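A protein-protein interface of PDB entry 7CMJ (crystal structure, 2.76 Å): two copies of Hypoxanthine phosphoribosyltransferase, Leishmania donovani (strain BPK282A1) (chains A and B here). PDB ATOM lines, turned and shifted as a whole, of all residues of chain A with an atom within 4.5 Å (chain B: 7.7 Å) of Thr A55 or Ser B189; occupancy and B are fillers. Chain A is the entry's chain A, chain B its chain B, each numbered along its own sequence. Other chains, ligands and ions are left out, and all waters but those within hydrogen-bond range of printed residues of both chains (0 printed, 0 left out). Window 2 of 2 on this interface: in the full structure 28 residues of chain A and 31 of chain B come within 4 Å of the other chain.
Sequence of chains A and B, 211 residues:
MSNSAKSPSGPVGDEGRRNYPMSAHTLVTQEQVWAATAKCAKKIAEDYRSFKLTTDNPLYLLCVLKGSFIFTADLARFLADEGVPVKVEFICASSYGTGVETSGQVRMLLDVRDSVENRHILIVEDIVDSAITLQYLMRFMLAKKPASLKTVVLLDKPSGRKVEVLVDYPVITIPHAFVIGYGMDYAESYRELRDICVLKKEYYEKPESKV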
ATOM      1  N   THR A  54       7.602  18.144  15.838  1.00  0.00           N
ATOM      2  CA  THR A  54       6.363  18.542  16.483  1.00  0.00           C
ATOM      3  C   THR A  54       6.643  19.760  17.354  1.00  0.00           C
ATOM      4  O   THR A  54       7.789  20.173  17.528  1.00  0.00           O
ATOM      5  CB  THR A  54       5.819  17.380  17.334  1.00  0.00           C
ATOM      6  OG1 THR A  54       5.924  16.159  16.593  1.00  0.00           O
ATOM      7  CG2 THR A  54       4.365  17.586  17.718  1.00  0.00           C
ATOM      8  N   THR A  55       5.585  20.351  17.904  1.00  0.00           N
ATOM      9  CA  THR A  55       5.782  21.292  19.001  1.00  0.00           C
ATOM     10  C   THR A  55       6.443  20.603  20.190  1.00  0.00           C
ATOM     11  O   THR A  55       7.350  21.160  20.813  1.00  0.00           O
ATOM     12  CB  THR A  55       4.446  21.915  19.405  1.00  0.00           C
ATOM     13  OG1 THR A  55       4.079  22.914  18.449  1.00  0.00           O
ATOM     14  CG2 THR A  55       4.537  22.546  20.762  1.00  0.00           C
ATOM     15  N   ASP A  56       6.022  19.376  20.500  1.00  0.00           N
ATOM     16  CA  ASP A  56       6.569  18.629  21.625  1.00  0.00           C
ATOM     17  C   ASP A  56       7.918  17.977  21.319  1.00  0.00           C
ATOM     18  O   ASP A  56       8.574  17.486  22.246  1.00  0.00           O
ATOM     19  CB  ASP A  56       5.568  17.557  22.079  1.00  0.00           C
ATOM     20  CG  ASP A  56       4.313  18.145  22.712  1.00  0.00           C
ATOM     21  OD1 ASP A  56       3.369  17.369  22.971  1.00  0.00           O
ATOM     22  OD2 ASP A  56       4.264  19.373  22.948  1.00  0.00           O
ATOM     23  N   ASN A  57       8.343  17.935  20.058  1.00  0.00           N
ATOM     24  CA  ASN A  57       9.693  17.497  19.695  1.00  0.00           C
ATOM     25  C   ASN A  57      10.217  18.451  18.639  1.00  0.00           C
ATOM     26  O   ASN A  57      10.281  18.116  17.449  1.00  0.00           O
ATOM     27  CB  ASN A  57       9.705  16.050  19.189  1.00  0.00           C
ATOM     28  CG  ASN A  57      11.100  15.581  18.772  1.00  0.00           C
ATOM     29  OD1 ASN A  57      12.118  15.971  19.362  1.00  0.00           O
ATOM     30  ND2 ASN A  57      11.148  14.749  17.743  1.00  0.00           N
ATOM     31  N   PRO A  58      10.603  19.666  19.039  1.00  0.00           N
ATOM     32  CA  PRO A  58      11.010  20.670  18.051  1.00  0.00           C
ATOM     33  C   PRO A  58      12.507  20.665  17.775  1.00  0.00           C
ATOM     34  O   PRO A  58      13.252  19.810  18.266  1.00  0.00           O
ATOM     35  CB  PRO A  58      10.576  21.978  18.715  1.00  0.00           C
ATOM     36  CG  PRO A  58      10.874  21.712  20.172  1.00  0.00           C
ATOM     37  CD  PRO A  58      10.655  20.212  20.404  1.00  0.00           C
ATOM     38  N   PRO A  85       8.855  23.974  14.005  1.00  0.00           N
ATOM     39  CA  PRO A  85       8.692  24.290  15.432  1.00  0.00           C
ATOM     40  C   PRO A  85      10.048  24.427  16.110  1.00  0.00           C
ATOM     41  O   PRO A  85      10.934  23.585  15.932  1.00  0.00           O
ATOM     42  CB  PRO A  85       7.886  23.103  15.973  1.00  0.00           C
ATOM     43  CG  PRO A  85       8.056  22.005  14.946  1.00  0.00           C
ATOM     44  CD  PRO A  85       8.286  22.664  13.638  1.00  0.00           C
ATOM     45  N   VAL A  86      10.198  25.492  16.906  1.00  0.00           N
ATOM     46  CA  VAL A  86      11.460  25.850  17.557  1.00  0.00           C
ATOM     47  C   VAL A  86      11.312  25.950  19.080  1.00  0.00           C
ATOM     48  O   VAL A  86      10.229  26.215  19.610  1.00  0.00           O
ATOM     49  CB  VAL A  86      11.984  27.182  16.964  1.00  0.00           C
ATOM     50  CG1 VAL A  86      13.045  27.823  17.832  1.00  0.00           C
ATOM     51  CG2 VAL A  86      12.521  26.935  15.597  1.00  0.00           C
ATOM     52  N   LYS A  87      12.408  25.690  19.787  1.00  0.00           N
ATOM     53  CA  LYS A  87      12.640  26.215  21.128  1.00  0.00           C
ATOM     54  C   LYS A  87      14.031  26.840  21.150  1.00  0.00           C
ATOM     55  O   LYS A  87      14.880  26.533  20.304  1.00  0.00           O
ATOM     56  CB  LYS A  87      12.517  25.129  22.207  1.00  0.00           C
ATOM     57  CG  LYS A  87      11.130  24.552  22.278  1.00  0.00           C
ATOM     58  CD  LYS A  87      10.876  23.741  23.526  1.00  0.00           C
ATOM     59  CE  LYS A  87       9.420  23.338  23.623  1.00  0.00           C
ATOM     60  NZ  LYS A  87       9.266  22.078  24.396  1.00  0.00           N
ATOM     61  N   VAL B 179      -0.021  35.942  26.537  1.00  0.00           N
ATOM     62  CA  VAL B 179       0.468  36.213  25.192  1.00  0.00           C
ATOM     63  C   VAL B 179       1.607  35.262  24.846  1.00  0.00           C
ATOM     64  O   VAL B 179       2.262  34.681  25.719  1.00  0.00           O
ATOM     65  CB  VAL B 179       0.925  37.672  25.058  1.00  0.00           C
ATOM     66  CG1 VAL B 179      -0.191  38.592  25.494  1.00  0.00           C
ATOM     67  CG2 VAL B 179       2.188  37.898  25.898  1.00  0.00           C
ATOM     68  N   ILE B 180       1.841  35.108  23.541  1.00  0.00           N
ATOM     69  CA  ILE B 180       2.940  34.307  23.013  1.00  0.00           C
ATOM     70  C   ILE B 180       3.514  34.989  21.776  1.00  0.00           C
ATOM     71  O   ILE B 180       2.963  35.960  21.247  1.00  0.00           O
ATOM     72  CB  ILE B 180       2.506  32.874  22.645  1.00  0.00           C
ATOM     73  CG1 ILE B 180       1.294  32.925  21.715  1.00  0.00           C
ATOM     74  CG2 ILE B 180       2.182  32.069  23.877  1.00  0.00           C
ATOM     75  CD1 ILE B 180       0.928  31.585  21.116  1.00  0.00           C
ATOM     76  N   GLY B 181       4.630  34.440  21.309  1.00  0.00           N
ATOM     77  CA  GLY B 181       5.304  34.915  20.120  1.00  0.00           C
ATOM     78  C   GLY B 181       6.297  36.019  20.413  1.00  0.00           C
ATOM     79  O   GLY B 181       6.339  36.601  21.498  1.00  0.00           O
ATOM     80  N   GLY B 183       9.512  36.063  20.879  1.00  0.00           N
ATOM     81  CA  GLY B 183      10.383  35.725  21.982  1.00  0.00           C
ATOM     82  C   GLY B 183       9.671  35.183  23.206  1.00  0.00           C
ATOM     83  O   GLY B 183      10.312  34.559  24.066  1.00  0.00           O
ATOM     84  N   MET B 184       8.368  35.394  23.308  1.00  0.00           N
ATOM     85  CA  MET B 184       7.623  35.007  24.492  1.00  0.00           C
ATOM     86  C   MET B 184       7.018  33.622  24.298  1.00  0.00           C
ATOM     87  O   MET B 184       6.578  33.266  23.203  1.00  0.00           O
ATOM     88  CB  MET B 184       6.553  36.049  24.801  1.00  0.00           C
ATOM     89  CG  MET B 184       7.138  37.450  25.003  1.00  0.00           C
ATOM     90  SD  MET B 184       5.871  38.628  25.488  1.00  0.00           S
ATOM     91  CE  MET B 184       5.106  38.942  23.898  1.00  0.00           C
ATOM     92  N   ASP B 185       7.020  32.834  25.366  1.00  0.00           N
ATOM     93  CA  ASP B 185       6.678  31.428  25.298  1.00  0.00           C
ATOM     94  C   ASP B 185       5.384  31.138  26.036  1.00  0.00           C
ATOM     95  O   ASP B 185       4.920  31.917  26.879  1.00  0.00           O
ATOM     96  CB  ASP B 185       7.781  30.572  25.909  1.00  0.00           C
ATOM     97  CG  ASP B 185       7.666  30.508  27.414  1.00  0.00           C
ATOM     98  OD1 ASP B 185       7.447  29.388  27.941  1.00  0.00           O
ATOM     99  OD2 ASP B 185       7.777  31.584  28.059  1.00  0.00           O
ATOM    100  N   TYR B 186       4.795  30.005  25.664  1.00  0.00           N
ATOM    101  CA  TYR B 186       3.951  29.205  26.542  1.00  0.00           C
ATOM    102  C   TYR B 186       4.645  27.850  26.603  1.00  0.00           C
ATOM    103  O   TYR B 186       4.753  27.165  25.574  1.00  0.00           O
ATOM    104  CB  TYR B 186       2.520  29.097  25.994  1.00  0.00           C
ATOM    105  CG  TYR B 186       1.740  28.028  26.713  1.00  0.00           C
ATOM    106  CD1 TYR B 186       1.675  26.726  26.225  1.00  0.00           C
ATOM    107  CD2 TYR B 186       1.131  28.303  27.925  1.00  0.00           C
ATOM    108  CE1 TYR B 186       1.002  25.748  26.914  1.00  0.00           C
ATOM    109  CE2 TYR B 186       0.458  27.330  28.628  1.00  0.00           C
ATOM    110  CZ  TYR B 186       0.394  26.051  28.121  1.00  0.00           C
ATOM    111  OH  TYR B 186      -0.286  25.074  28.831  1.00  0.00           O
ATOM    112  N   ALA B 187       5.183  27.496  27.776  1.00  0.00           N
ATOM    113  CA  ALA B 187       5.890  26.204  27.976  1.00  0.00           C
ATOM    114  C   ALA B 187       7.081  26.020  27.020  1.00  0.00           C
ATOM    115  O   ALA B 187       7.276  24.944  26.449  1.00  0.00           O
ATOM    116  CB  ALA B 187       4.919  25.033  27.829  1.00  0.00           C
ATOM    117  N   GLU B 188       7.882  27.089  26.856  1.00  0.00           N
ATOM    118  CA  GLU B 188       9.068  27.137  25.988  1.00  0.00           C
ATOM    119  C   GLU B 188       8.745  27.091  24.493  1.00  0.00           C
ATOM    120  O   GLU B 188       9.626  27.335  23.663  1.00  0.00           O
ATOM    121  CB  GLU B 188      10.051  26.015  26.334  1.00  0.00           C
ATOM    122  CG  GLU B 188      10.641  26.137  27.723  1.00  0.00           C
ATOM    123  CD  GLU B 188      11.325  27.464  27.972  1.00  0.00           C
ATOM    124  OE1 GLU B 188      11.944  28.012  27.042  1.00  0.00           O
ATOM    125  OE2 GLU B 188      11.253  27.958  29.116  1.00  0.00           O
ATOM    126  N   SER B 189       7.500  26.807  24.133  1.00  0.00           N
ATOM    127  CA  SER B 189       7.091  26.833  22.738  1.00  0.00           C
ATOM    128  C   SER B 189       6.705  28.255  22.309  1.00  0.00           C
ATOM    129  O   SER B 189       6.399  29.126  23.136  1.00  0.00           O
ATOM    130  CB  SER B 189       5.918  25.873  22.514  1.00  0.00           C
ATOM    131  OG  SER B 189       6.379  24.568  22.184  1.00  0.00           O
ATOM    132  N   TYR B 190       6.747  28.482  20.991  1.00  0.00           N
ATOM    133  CA  TYR B 190       6.226  29.663  20.268  1.00  0.00           C
ATOM    134  C   TYR B 190       7.048  30.941  20.388  1.00  0.00           C
ATOM    135  O   TYR B 190       6.577  31.978  19.938  1.00  0.00           O
ATOM    136  CB  TYR B 190       4.790  30.021  20.667  1.00  0.00           C
ATOM    137  CG  TYR B 190       3.861  28.844  20.632  1.00  0.00           C
ATOM    138  CD1 TYR B 190       3.703  28.099  19.473  1.00  0.00           C
ATOM    139  CD2 TYR B 190       3.160  28.454  21.767  1.00  0.00           C
ATOM    140  CE1 TYR B 190       2.863  26.999  19.434  1.00  0.00           C
ATOM    141  CE2 TYR B 190       2.318  27.359  21.739  1.00  0.00           C
ATOM    142  CZ  TYR B 190       2.176  26.631  20.569  1.00  0.00           C
ATOM    143  OH  TYR B 190       1.345  25.537  20.527  1.00  0.00           O
ATOM    144  N   ARG B 191       8.256  30.914  20.948  1.00  0.00           N
ATOM    145  CA  ARG B 191       9.054  32.136  20.973  1.00  0.00           C
ATOM    146  C   ARG B 191       9.362  32.639  19.573  1.00  0.00           C
ATOM    147  O   ARG B 191       9.618  33.838  19.395  1.00  0.00           O
ATOM    148  CB  ARG B 191      10.366  31.906  21.732  1.00  0.00           C
ATOM    149  CG  ARG B 191      10.209  31.434  23.179  1.00  0.00           C
ATOM    150  CD  ARG B 191      11.539  31.474  23.897  1.00  0.00           C
ATOM    151  NE  ARG B 191      11.463  30.860  25.222  1.00  0.00           N
ATOM    152  CZ  ARG B 191      10.957  31.460  26.293  1.00  0.00           C
ATOM    153  NH1 ARG B 191      10.480  32.699  26.204  1.00  0.00           N
ATOM    154  NH2 ARG B 191      10.921  30.823  27.449  1.00  0.00           N
ATOM    155  N   GLU B 192       9.295  31.760  18.572  1.00  0.00           N
ATOM    156  CA  GLU B 192       9.820  32.021  17.239  1.00  0.00           C
ATOM    157  C   GLU B 192       8.841  32.752  16.323  1.00  0.00           C
ATOM    158  O   GLU B 192       9.238  33.130  15.213  1.00  0.00           O
ATOM    159  CB  GLU B 192      10.260  30.693  16.590  1.00  0.00           C
ATOM    160  CG  GLU B 192       9.117  29.760  16.155  1.00  0.00           C
ATOM    161  CD  GLU B 192       8.601  28.838  17.262  1.00  0.00           C
ATOM    162  OE1 GLU B 192       8.033  27.767  16.950  1.00  0.00           O
ATOM    163  OE2 GLU B 192       8.746  29.181  18.447  1.00  0.00           O
ATOM    164  N   LEU B 193       7.600  32.985  16.764  1.00  0.00           N
ATOM    165  CA  LEU B 193       6.581  33.593  15.905  1.00  0.00           C
ATOM    166  C   LEU B 193       6.821  35.089  15.703  1.00  0.00           C
ATOM    167  O   LEU B 193       7.214  35.798  16.632  1.00  0.00           O
ATOM    168  CB  LEU B 193       5.192  33.369  16.494  1.00  0.00           C
ATOM    169  CG  LEU B 193       4.799  31.938  16.874  1.00  0.00           C
ATOM    170  CD1 LEU B 193       3.333  31.892  17.261  1.00  0.00           C
ATOM    171  CD2 LEU B 193       5.082  30.943  15.755  1.00  0.00           C
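The backbone NH (N) of Val A86 is in hydrogen-bond range of the side-chain carboxylate (OE1) of Glu B192.
The backbone NH (N) of Tyr B190 sits close to the side-chain carboxylate (OE2) of Glu B192, 3.3 Å away.
The side-chain carboxylate (OD1) of Asp B185 is in hydrogen-bond range of the backbone NH (N) of Glu B188.
The side-chain carboxylate (OE1) of Glu B188 lies within salt-bridge range of the guanidinium group (NH2) of Arg B191 (3.0 Å).
The backbone NH (N) of Ala B187 lies within hydrogen-bond range of the side-chain carboxylate (OD1) of Asp B185 (3.0 Å).
OG of Ser B189 touches CG2 of Thr A55 (3.1 Å).
Pro A85 touches Glu B192.
Lys A87 touches Ala B187 (CE to O, 3.9 Å).
O of Glu B188 touches CG of Lys A87, at 3.5 Å.
CE of Lys A87 touches OG of Ser B189 (3.6 Å).
Thr A55 touches just one residue of chain B: Ser B189 (3.1 Å).
Ser B189 touches just these residues of chain A: Thr A55 (3.1 Å) and Lys A87 (3.6 Å).
Printed residues of chain A within 4 Å of Glu B192: Pro A85 and Val A86.
Printed residues of chain B within 4 Å of Pro A85: Glu B192.
Printed residues of chain B within 4 Å of Val A86: Glu B192 (3.1 Å).
Printed residues of chain B within 4 Å of Lys A87: Ala B187 (3.9 Å), Glu B188 (3.5 Å) and Ser B189 (3.6 Å).
Of the printed residues of chain A, Ala B187 touches Lys A87.
Leu B193 touches none of the printed residues of chain A.
The nearest residue of chain B that does not touch Thr A55 is Tyr B190 (4.3 Å).
Along chain B the printed residues that touch a printed residue of chain A span positions 187 to 192.
Printed residues of chain A that touch a printed residue of chain B: Thr A55, Pro A85, Val A86 and Lys A87.
Hydrophobic or aromatic side chains of chain A within 4 Å of the printed part of chain B: Val A86.
No position is printed for both chains.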
